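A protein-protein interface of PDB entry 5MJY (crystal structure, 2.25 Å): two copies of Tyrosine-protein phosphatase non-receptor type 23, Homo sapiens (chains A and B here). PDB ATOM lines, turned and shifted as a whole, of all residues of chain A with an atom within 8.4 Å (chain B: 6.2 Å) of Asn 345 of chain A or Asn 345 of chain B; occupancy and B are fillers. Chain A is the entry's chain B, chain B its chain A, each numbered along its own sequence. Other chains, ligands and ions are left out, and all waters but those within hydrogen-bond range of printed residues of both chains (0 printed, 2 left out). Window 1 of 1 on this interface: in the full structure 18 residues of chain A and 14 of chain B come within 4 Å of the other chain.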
ATOM      1  N   ARG A  69      23.473 -34.728 -22.901  1.00  0.00           N
ATOM      2  CA  ARG A  69      23.429 -34.101 -21.584  1.00  0.00           C
ATOM      3  C   ARG A  69      22.587 -34.918 -20.613  1.00  0.00           C
ATOM      4  O   ARG A  69      22.992 -35.137 -19.466  1.00  0.00           O
ATOM      5  CB  ARG A  69      22.888 -32.673 -21.689  1.00  0.00           C
ATOM      6  CG  ARG A  69      23.888 -31.651 -22.214  1.00  0.00           C
ATOM      7  CD  ARG A  69      25.026 -31.400 -21.223  1.00  0.00           C
ATOM      8  NE  ARG A  69      24.557 -30.805 -19.974  1.00  0.00           N
ATOM      9  CZ  ARG A  69      24.463 -29.497 -19.744  1.00  0.00           C
ATOM     10  NH1 ARG A  69      24.803 -28.620 -20.679  1.00  0.00           N
ATOM     11  NH2 ARG A  69      24.022 -29.062 -18.571  1.00  0.00           N
ATOM     12  N   LEU A  72      24.407 -38.034 -19.650  1.00  0.00           N
ATOM     13  CA  LEU A  72      25.486 -37.640 -18.750  1.00  0.00           C
ATOM     14  C   LEU A  72      24.963 -37.416 -17.338  1.00  0.00           C
ATOM     15  O   LEU A  72      25.594 -37.833 -16.360  1.00  0.00           O
ATOM     16  CB  LEU A  72      26.172 -36.377 -19.270  1.00  0.00           C
ATOM     17  CG  LEU A  72      27.248 -35.759 -18.369  1.00  0.00           C
ATOM     18  CD1 LEU A  72      28.366 -36.748 -18.080  1.00  0.00           C
ATOM     19  CD2 LEU A  72      27.810 -34.494 -19.005  1.00  0.00           C
ATOM     20  N   GLY A  73      23.811 -36.758 -17.211  1.00  0.00           N
ATOM     21  CA  GLY A  73      23.260 -36.501 -15.892  1.00  0.00           C
ATOM     22  C   GLY A  73      22.799 -37.766 -15.194  1.00  0.00           C
ATOM     23  O   GLY A  73      23.032 -37.943 -13.996  1.00  0.00           O
ATOM     24  N   HIS A  76      25.516 -39.536 -13.507  1.00  0.00           N
ATOM     25  CA  HIS A  76      25.827 -38.943 -12.209  1.00  0.00           C
ATOM     26  C   HIS A  76      24.853 -39.423 -11.140  1.00  0.00           C
ATOM     27  O   HIS A  76      25.262 -39.768 -10.024  1.00  0.00           O
ATOM     28  CB  HIS A  76      25.808 -37.416 -12.305  1.00  0.00           C
ATOM     29  CG  HIS A  76      27.075 -36.825 -12.840  1.00  0.00           C
ATOM     30  ND1 HIS A  76      27.395 -36.836 -14.181  1.00  0.00           N
ATOM     31  CD2 HIS A  76      28.104 -36.206 -12.214  1.00  0.00           C
ATOM     32  CE1 HIS A  76      28.566 -36.249 -14.358  1.00  0.00           C
ATOM     33  NE2 HIS A  76      29.017 -35.858 -13.180  1.00  0.00           N
ATOM     34  N   TYR A  77      23.558 -39.453 -11.463  1.00  0.00           N
ATOM     35  CA  TYR A  77      22.568 -39.938 -10.505  1.00  0.00           C
ATOM     36  C   TYR A  77      22.812 -41.398 -10.143  1.00  0.00           C
ATOM     37  O   TYR A  77      22.689 -41.784  -8.974  1.00  0.00           O
ATOM     38  CB  TYR A  77      21.160 -39.751 -11.072  1.00  0.00           C
ATOM     39  CG  TYR A  77      20.784 -38.309 -11.329  1.00  0.00           C
ATOM     40  CD1 TYR A  77      21.247 -37.292 -10.504  1.00  0.00           C
ATOM     41  CD2 TYR A  77      19.970 -37.962 -12.399  1.00  0.00           C
ATOM     42  CE1 TYR A  77      20.909 -35.974 -10.735  1.00  0.00           C
ATOM     43  CE2 TYR A  77      19.625 -36.644 -12.638  1.00  0.00           C
ATOM     44  CZ  TYR A  77      20.099 -35.654 -11.800  1.00  0.00           C
ATOM     45  OH  TYR A  77      19.766 -34.336 -12.023  1.00  0.00           O
ATOM     46  N   LEU A 118      30.886 -36.795 -22.442  1.00  0.00           N
ATOM     47  CA  LEU A 118      31.174 -35.368 -22.441  1.00  0.00           C
ATOM     48  C   LEU A 118      32.054 -34.991 -23.626  1.00  0.00           C
ATOM     49  O   LEU A 118      31.875 -33.926 -24.228  1.00  0.00           O
ATOM     50  CB  LEU A 118      31.838 -34.975 -21.122  1.00  0.00           C
ATOM     51  CG  LEU A 118      31.954 -33.479 -20.834  1.00  0.00           C
ATOM     52  CD1 LEU A 118      30.590 -32.802 -20.844  1.00  0.00           C
ATOM     53  CD2 LEU A 118      32.638 -33.269 -19.499  1.00  0.00           C
ATOM     54  N   LEU A 121      29.815 -34.843 -26.583  1.00  0.00           N
ATOM     55  CA  LEU A 121      29.024 -33.620 -26.538  1.00  0.00           C
ATOM     56  C   LEU A 121      29.801 -32.457 -27.139  1.00  0.00           C
ATOM     57  O   LEU A 121      29.259 -31.675 -27.929  1.00  0.00           O
ATOM     58  CB  LEU A 121      28.612 -33.309 -25.099  1.00  0.00           C
ATOM     59  CG  LEU A 121      27.806 -32.023 -24.898  1.00  0.00           C
ATOM     60  CD1 LEU A 121      26.481 -32.084 -25.644  1.00  0.00           C
ATOM     61  CD2 LEU A 121      27.575 -31.756 -23.417  1.00  0.00           C
ATOM     62  N   GLY A 152      33.211 -25.530 -23.918  1.00  0.00           N
ATOM     63  CA  GLY A 152      32.807 -25.752 -22.539  1.00  0.00           C
ATOM     64  C   GLY A 152      32.822 -27.219 -22.157  1.00  0.00           C
ATOM     65  O   GLY A 152      33.142 -27.572 -21.019  1.00  0.00           O
ATOM     66  N   TYR A 156      35.385 -28.512 -19.265  1.00  0.00           N
ATOM     67  CA  TYR A 156      34.915 -29.276 -18.113  1.00  0.00           C
ATOM     68  C   TYR A 156      35.627 -30.618 -18.026  1.00  0.00           C
ATOM     69  O   TYR A 156      36.055 -31.037 -16.944  1.00  0.00           O
ATOM     70  CB  TYR A 156      33.404 -29.478 -18.203  1.00  0.00           C
ATOM     71  CG  TYR A 156      32.779 -30.063 -16.955  1.00  0.00           C
ATOM     72  CD1 TYR A 156      32.788 -31.434 -16.723  1.00  0.00           C
ATOM     73  CD2 TYR A 156      32.168 -29.247 -16.014  1.00  0.00           C
ATOM     74  CE1 TYR A 156      32.214 -31.971 -15.586  1.00  0.00           C
ATOM     75  CE2 TYR A 156      31.591 -29.774 -14.876  1.00  0.00           C
ATOM     76  CZ  TYR A 156      31.616 -31.136 -14.667  1.00  0.00           C
ATOM     77  OH  TYR A 156      31.043 -31.665 -13.534  1.00  0.00           O
ATOM     78  N   HIS A 160      37.622 -31.477 -14.557  1.00  0.00           N
ATOM     79  CA  HIS A 160      36.999 -32.411 -13.627  1.00  0.00           C
ATOM     80  C   HIS A 160      37.377 -33.865 -13.873  1.00  0.00           C
ATOM     81  O   HIS A 160      37.006 -34.725 -13.068  1.00  0.00           O
ATOM     82  CB  HIS A 160      35.476 -32.265 -13.686  1.00  0.00           C
ATOM     83  CG  HIS A 160      34.978 -30.977 -13.111  1.00  0.00           C
ATOM     84  ND1 HIS A 160      34.644 -30.837 -11.781  1.00  0.00           N
ATOM     85  CD2 HIS A 160      34.771 -29.767 -13.681  1.00  0.00           C
ATOM     86  CE1 HIS A 160      34.242 -29.599 -11.559  1.00  0.00           C
ATOM     87  NE2 HIS A 160      34.312 -28.928 -12.694  1.00  0.00           N
ATOM     88  N   LEU A 342      31.488 -22.282 -22.341  1.00  0.00           N
ATOM     89  CA  LEU A 342      30.275 -22.151 -21.548  1.00  0.00           C
ATOM     90  C   LEU A 342      30.234 -23.240 -20.481  1.00  0.00           C
ATOM     91  O   LEU A 342      30.360 -24.426 -20.810  1.00  0.00           O
ATOM     92  CB  LEU A 342      29.043 -22.217 -22.447  1.00  0.00           C
ATOM     93  CG  LEU A 342      29.011 -21.091 -23.486  1.00  0.00           C
ATOM     94  CD1 LEU A 342      27.858 -21.275 -24.454  1.00  0.00           C
ATOM     95  CD2 LEU A 342      28.942 -19.705 -22.832  1.00  0.00           C
ATOM     96  N   PRO A 343      30.063 -22.891 -19.204  1.00  0.00           N
ATOM     97  CA  PRO A 343      30.127 -23.912 -18.154  1.00  0.00           C
ATOM     98  C   PRO A 343      29.017 -24.941 -18.297  1.00  0.00           C
ATOM     99  O   PRO A 343      27.936 -24.659 -18.819  1.00  0.00           O
ATOM    100  CB  PRO A 343      29.973 -23.107 -16.858  1.00  0.00           C
ATOM    101  CG  PRO A 343      30.242 -21.688 -17.235  1.00  0.00           C
ATOM    102  CD  PRO A 343      29.815 -21.550 -18.649  1.00  0.00           C
ATOM    103  N   VAL A 344      29.304 -26.148 -17.818  1.00  0.00           N
ATOM    104  CA  VAL A 344      28.367 -27.265 -17.835  1.00  0.00           C
ATOM    105  C   VAL A 344      28.052 -27.643 -16.394  1.00  0.00           C
ATOM    106  O   VAL A 344      28.964 -27.784 -15.570  1.00  0.00           O
ATOM    107  CB  VAL A 344      28.942 -28.471 -18.602  1.00  0.00           C
ATOM    108  CG1 VAL A 344      28.129 -29.738 -18.334  1.00  0.00           C
ATOM    109  CG2 VAL A 344      28.981 -28.175 -20.093  1.00  0.00           C
ATOM    110  N   ASN A 345      26.762 -27.807 -16.094  1.00  0.00           N
ATOM    111  CA  ASN A 345      26.315 -28.374 -14.825  1.00  0.00           C
ATOM    112  C   ASN A 345      25.680 -29.726 -15.124  1.00  0.00           C
ATOM    113  O   ASN A 345      24.483 -29.800 -15.437  1.00  0.00           O
ATOM    114  CB  ASN A 345      25.323 -27.451 -14.115  1.00  0.00           C
ATOM    115  CG  ASN A 345      24.884 -28.000 -12.771  1.00  0.00           C
ATOM    116  OD1 ASN A 345      25.334 -29.066 -12.347  1.00  0.00           O
ATOM    117  ND2 ASN A 345      24.008 -27.271 -12.092  1.00  0.00           N
ATOM    118  N   PRO A 346      26.433 -30.826 -15.047  1.00  0.00           N
ATOM    119  CA  PRO A 346      25.881 -32.117 -15.494  1.00  0.00           C
ATOM    120  C   PRO A 346      24.598 -32.516 -14.785  1.00  0.00           C
ATOM    121  O   PRO A 346      23.774 -33.223 -15.376  1.00  0.00           O
ATOM    122  CB  PRO A 346      27.019 -33.106 -15.202  1.00  0.00           C
ATOM    123  CG  PRO A 346      28.248 -32.277 -15.106  1.00  0.00           C
ATOM    124  CD  PRO A 346      27.816 -30.955 -14.560  1.00  0.00           C
ATOM    125  N   THR A 347      24.390 -32.070 -13.544  1.00  0.00           N
ATOM    126  CA  THR A 347      23.239 -32.483 -12.750  1.00  0.00           C
ATOM    127  C   THR A 347      22.177 -31.393 -12.646  1.00  0.00           C
ATOM    128  O   THR A 347      21.375 -31.401 -11.707  1.00  0.00           O
ATOM    129  CB  THR A 347      23.689 -32.918 -11.354  1.00  0.00           C
ATOM    130  OG1 THR A 347      24.557 -31.925 -10.791  1.00  0.00           O
ATOM    131  CG2 THR A 347      24.419 -34.257 -11.427  1.00  0.00           C
ATOM    132  N   ASP A 348      22.147 -30.462 -13.596  1.00  0.00           N
ATOM    133  CA  ASP A 348      21.083 -29.469 -13.664  1.00  0.00           C
ATOM    134  C   ASP A 348      19.762 -30.182 -13.947  1.00  0.00           C
ATOM    135  O   ASP A 348      19.599 -30.756 -15.031  1.00  0.00           O
ATOM    136  CB  ASP A 348      21.388 -28.434 -14.750  1.00  0.00           C
ATOM    137  CG  ASP A 348      20.404 -27.281 -14.755  1.00  0.00           C
ATOM    138  OD1 ASP A 348      19.238 -27.480 -14.358  1.00  0.00           O
ATOM    139  OD2 ASP A 348      20.800 -26.169 -15.160  1.00  0.00           O
ATOM    140  N   PRO A 349      18.799 -30.178 -13.018  1.00  0.00           N
ATOM    141  CA  PRO A 349      17.547 -30.913 -13.276  1.00  0.00           C
ATOM    142  C   PRO A 349      16.819 -30.457 -14.527  1.00  0.00           C
ATOM    143  O   PRO A 349      16.101 -31.257 -15.140  1.00  0.00           O
ATOM    144  CB  PRO A 349      16.714 -30.645 -12.015  1.00  0.00           C
ATOM    145  CG  PRO A 349      17.705 -30.274 -10.968  1.00  0.00           C
ATOM    146  CD  PRO A 349      18.802 -29.554 -11.684  1.00  0.00           C
ATOM    147  N   ALA A 350      16.984 -29.196 -14.930  1.00  0.00           N
ATOM    148  CA  ALA A 350      16.280 -28.688 -16.102  1.00  0.00           C
ATOM    149  C   ALA A 350      16.749 -29.340 -17.397  1.00  0.00           C
ATOM    150  O   ALA A 350      16.013 -29.310 -18.390  1.00  0.00           O
ATOM    151  CB  ALA A 350      16.447 -27.170 -16.193  1.00  0.00           C
ATOM    152  N   VAL A 351      17.947 -29.924 -17.417  1.00  0.00           N
ATOM    153  CA  VAL A 351      18.451 -30.592 -18.605  1.00  0.00           C
ATOM    154  C   VAL A 351      18.464 -32.111 -18.452  1.00  0.00           C
ATOM    155  O   VAL A 351      18.379 -32.822 -19.459  1.00  0.00           O
ATOM    156  CB  VAL A 351      19.857 -30.072 -18.987  1.00  0.00           C
ATOM    157  CG1 VAL A 351      20.097 -28.675 -18.423  1.00  0.00           C
ATOM    158  CG2 VAL A 351      20.967 -31.033 -18.538  1.00  0.00           C
ATOM    159  N   THR A 352      18.571 -32.627 -17.228  1.00  0.00           N
ATOM    160  CA  THR A 352      18.607 -34.067 -17.004  1.00  0.00           C
ATOM    161  C   THR A 352      17.225 -34.692 -16.907  1.00  0.00           C
ATOM    162  O   THR A 352      17.093 -35.904 -17.110  1.00  0.00           O
ATOM    163  CB  THR A 352      19.373 -34.386 -15.715  1.00  0.00           C
ATOM    164  OG1 THR A 352      18.652 -33.876 -14.582  1.00  0.00           O
ATOM    165  CG2 THR A 352      20.765 -33.771 -15.748  1.00  0.00           C
ATOM    166  N   ARG B  69      25.583 -17.546  -4.309  1.00  0.00           N
ATOM    167  CA  ARG B  69      26.046 -18.195  -5.531  1.00  0.00           C
ATOM    168  C   ARG B  69      26.256 -17.180  -6.647  1.00  0.00           C
ATOM    169  O   ARG B  69      27.290 -17.188  -7.325  1.00  0.00           O
ATOM    170  CB  ARG B  69      25.037 -19.257  -5.966  1.00  0.00           C
ATOM    171  CG  ARG B  69      25.574 -20.673  -5.971  1.00  0.00           C
ATOM    172  CD  ARG B  69      24.433 -21.675  -6.034  1.00  0.00           C
ATOM    173  NE  ARG B  69      24.461 -22.601  -4.907  1.00  0.00           N
ATOM    174  CZ  ARG B  69      23.407 -23.274  -4.457  1.00  0.00           C
ATOM    175  NH1 ARG B  69      22.215 -23.127  -5.024  1.00  0.00           N
ATOM    176  NH2 ARG B  69      23.545 -24.094  -3.426  1.00  0.00           N
ATOM    177  N   TYR B 156      34.922 -28.113  -1.186  1.00  0.00           N
ATOM    178  CA  TYR B 156      35.506 -27.262  -2.217  1.00  0.00           C
ATOM    179  C   TYR B 156      36.495 -26.277  -1.611  1.00  0.00           C
ATOM    180  O   TYR B 156      37.598 -26.085  -2.137  1.00  0.00           O
ATOM    181  CB  TYR B 156      34.397 -26.518  -2.964  1.00  0.00           C
ATOM    182  CG  TYR B 156      34.855 -25.782  -4.204  1.00  0.00           C
ATOM    183  CD1 TYR B 156      35.485 -24.549  -4.111  1.00  0.00           C
ATOM    184  CD2 TYR B 156      34.642 -26.312  -5.469  1.00  0.00           C
ATOM    185  CE1 TYR B 156      35.901 -23.870  -5.241  1.00  0.00           C
ATOM    186  CE2 TYR B 156      35.055 -25.642  -6.605  1.00  0.00           C
ATOM    187  CZ  TYR B 156      35.683 -24.419  -6.484  1.00  0.00           C
ATOM    188  OH  TYR B 156      36.097 -23.743  -7.609  1.00  0.00           O
ATOM    189  N   PRO B 343      28.768 -31.115  -5.539  1.00  0.00           N
ATOM    190  CA  PRO B 343      29.566 -30.069  -6.193  1.00  0.00           C
ATOM    191  C   PRO B 343      28.909 -28.700  -6.075  1.00  0.00           C
ATOM    192  O   PRO B 343      27.685 -28.575  -6.025  1.00  0.00           O
ATOM    193  CB  PRO B 343      29.640 -30.537  -7.651  1.00  0.00           C
ATOM    194  CG  PRO B 343      29.390 -32.002  -7.595  1.00  0.00           C
ATOM    195  CD  PRO B 343      28.427 -32.206  -6.470  1.00  0.00           C
ATOM    196  N   VAL B 344      29.747 -27.666  -6.036  1.00  0.00           N
ATOM    197  CA  VAL B 344      29.271 -26.300  -5.843  1.00  0.00           C
ATOM    198  C   VAL B 344      28.916 -25.638  -7.170  1.00  0.00           C
ATOM    199  O   VAL B 344      27.955 -24.867  -7.247  1.00  0.00           O
ATOM    200  CB  VAL B 344      30.331 -25.492  -5.066  1.00  0.00           C
ATOM    201  CG1 VAL B 344      30.009 -23.998  -5.078  1.00  0.00           C
ATOM    202  CG2 VAL B 344      30.428 -25.998  -3.632  1.00  0.00           C
ATOM    203  N   ASN B 345      29.671 -25.927  -8.233  1.00  0.00           N
ATOM    204  CA  ASN B 345      29.469 -25.285  -9.527  1.00  0.00           C
ATOM    205  C   ASN B 345      29.468 -23.769  -9.364  1.00  0.00           C
ATOM    206  O   ASN B 345      28.412 -23.132  -9.463  1.00  0.00           O
ATOM    207  CB  ASN B 345      28.164 -25.761 -10.169  1.00  0.00           C
ATOM    208  CG  ASN B 345      28.371 -26.938 -11.103  1.00  0.00           C
ATOM    209  OD1 ASN B 345      28.695 -26.759 -12.277  1.00  0.00           O
ATOM    210  ND2 ASN B 345      28.190 -28.149 -10.585  1.00  0.00           N
ATOM    211  N   PRO B 346      30.630 -23.152  -9.122  1.00  0.00           N
ATOM    212  CA  PRO B 346      30.635 -21.711  -8.820  1.00  0.00           C
ATOM    213  C   PRO B 346      30.241 -20.833  -9.995  1.00  0.00           C
ATOM    214  O   PRO B 346      29.670 -19.758  -9.778  1.00  0.00           O
ATOM    215  CB  PRO B 346      32.086 -21.444  -8.385  1.00  0.00           C
ATOM    216  CG  PRO B 346      32.687 -22.789  -8.123  1.00  0.00           C
ATOM    217  CD  PRO B 346      31.974 -23.740  -9.023  1.00  0.00           C
ATOM    218  N   THR B 347      30.528 -21.247 -11.230  1.00  0.00           N
ATOM    219  CA  THR B 347      30.287 -20.421 -12.409  1.00  0.00           C
ATOM    220  C   THR B 347      29.118 -20.934 -13.245  1.00  0.00           C
ATOM    221  O   THR B 347      29.080 -20.727 -14.460  1.00  0.00           O
ATOM    222  CB  THR B 347      31.551 -20.335 -13.262  1.00  0.00           C
ATOM    223  OG1 THR B 347      32.109 -21.644 -13.428  1.00  0.00           O
ATOM    224  CG2 THR B 347      32.580 -19.419 -12.609  1.00  0.00           C
ATOM    225  N   ASP B 348      28.154 -21.593 -12.611  1.00  0.00           N
ATOM    226  CA  ASP B 348      26.963 -22.065 -13.307  1.00  0.00           C
ATOM    227  C   ASP B 348      26.180 -20.872 -13.851  1.00  0.00           C
ATOM    228  O   ASP B 348      25.626 -20.094 -13.063  1.00  0.00           O
ATOM    229  CB  ASP B 348      26.094 -22.898 -12.363  1.00  0.00           C
ATOM    230  CG  ASP B 348      24.906 -23.530 -13.062  1.00  0.00           C
ATOM    231  OD1 ASP B 348      24.501 -23.030 -14.132  1.00  0.00           O
ATOM    232  OD2 ASP B 348      24.373 -24.530 -12.537  1.00  0.00           O
ATOM    233  N   VAL B 351      22.731 -19.828 -12.417  1.00  0.00           N
ATOM    234  CA  VAL B 351      22.620 -19.152 -11.135  1.00  0.00           C
ATOM    235  C   VAL B 351      23.374 -17.824 -11.109  1.00  0.00           C
ATOM    236  O   VAL B 351      22.989 -16.924 -10.356  1.00  0.00           O
ATOM    237  CB  VAL B 351      23.097 -20.069  -9.988  1.00  0.00           C
ATOM    238  CG1 VAL B 351      24.619 -20.194  -9.978  1.00  0.00           C
ATOM    239  CG2 VAL B 351      22.582 -19.561  -8.650  1.00  0.00           C
ATOM    240  N   THR B 352      24.438 -17.676 -11.903  1.00  0.00           N
ATOM    241  CA  THR B 352      25.222 -16.446 -11.891  1.00  0.00           C
ATOM    242  C   THR B 352      24.631 -15.374 -12.797  1.00  0.00           C
ATOM    243  O   THR B 352      24.846 -14.181 -12.557  1.00  0.00           O
ATOM    244  CB  THR B 352      26.662 -16.729 -12.325  1.00  0.00           C
ATOM    245  OG1 THR B 352      26.677 -17.152 -13.694  1.00  0.00           O
ATOM    246  CG2 THR B 352      27.290 -17.808 -11.450  1.00  0.00           C
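OD1 of Asn 345 of chain B lies close to O of Val 344 of chain A (3.5 Å).
The side-chain amide nitrogen (ND2) of Asn 345 of chain B sits at hydrogen-bond distance from the side-chain amide oxygen (OD1) of Asn 345 of chain A (3.5 Å).
The side-chain carboxylate of Asp 348 of chain B sits at hydrogen-bond distance from the side-chain amide nitrogen of Asn 345 of chain A (2.8 Å).
The backbone carbonyl oxygen of Asp 348 of chain B lies within hydrogen-bond range of the side-chain hydroxyl of Thr 352 of chain B (3.2 Å).
The backbone carbonyl oxygen (O) of Asn 345 of chain A is in hydrogen-bond range of the guanidinium group (NH2) of Arg 69 of chain A, 3.3 Å away.
OG1 of Thr 347 of chain A lies within hydrogen-bond range of OD1 of Asn 345 of chain A, 3.3 Å away.
Thr 347 of chain B touches Pro 343 of chain A.
Gly 152 of chain A touches none of the printed residues of chain B.
Leu 342 of chain A touches none of the printed residues of chain B.
Printed residues of chain B within 4 Å of Val 344 of chain A: Asn 345.
Asn 345 of chain A touches just these residues of chain B: Asn 345 and Asp 348.
No residue of chain A comes within 4 Å of Pro 346 of chain B.
Printed residues of chain A within 4 Å of Thr 347 of chain B: Pro 343.
The nearest printed residue of chain B that does not touch Asn 345 of chain A is Pro 343 of chain B (6.5 Å).
The nearest printed residue of chain B that does not touch Pro 343 of chain A is Asp 348 of chain B (4.8 Å).
Hydrophobic or aromatic side chains of chain A that line the printed part of chain B: Pro 343.
Among the printed residues, no Asp or Glu carboxylate lies within 4 Å of a Lys or Arg side-chain nitrogen of the other chain.
Pro 343 of chain A touches Thr 347 of chain B, but with the chains exchanged Thr 347 of chain A does not touch Pro 343 of chain B (5.8 Å).
Val 344 of chain A touches Asn 345 of chain B, but with the chains exchanged Asn 345 of chain A does not touch Val 344 of chain B (6.7 Å).
Asn 345 of chain A touches its own counterpart, Asn 345 of chain B.
Asn 345 of chain A touches Asp 348 of chain B, but with the chains exchanged Asp 348 of chain A does not touch Asn 345 of chain B (7.1 Å).
10 positions are printed for both chains.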
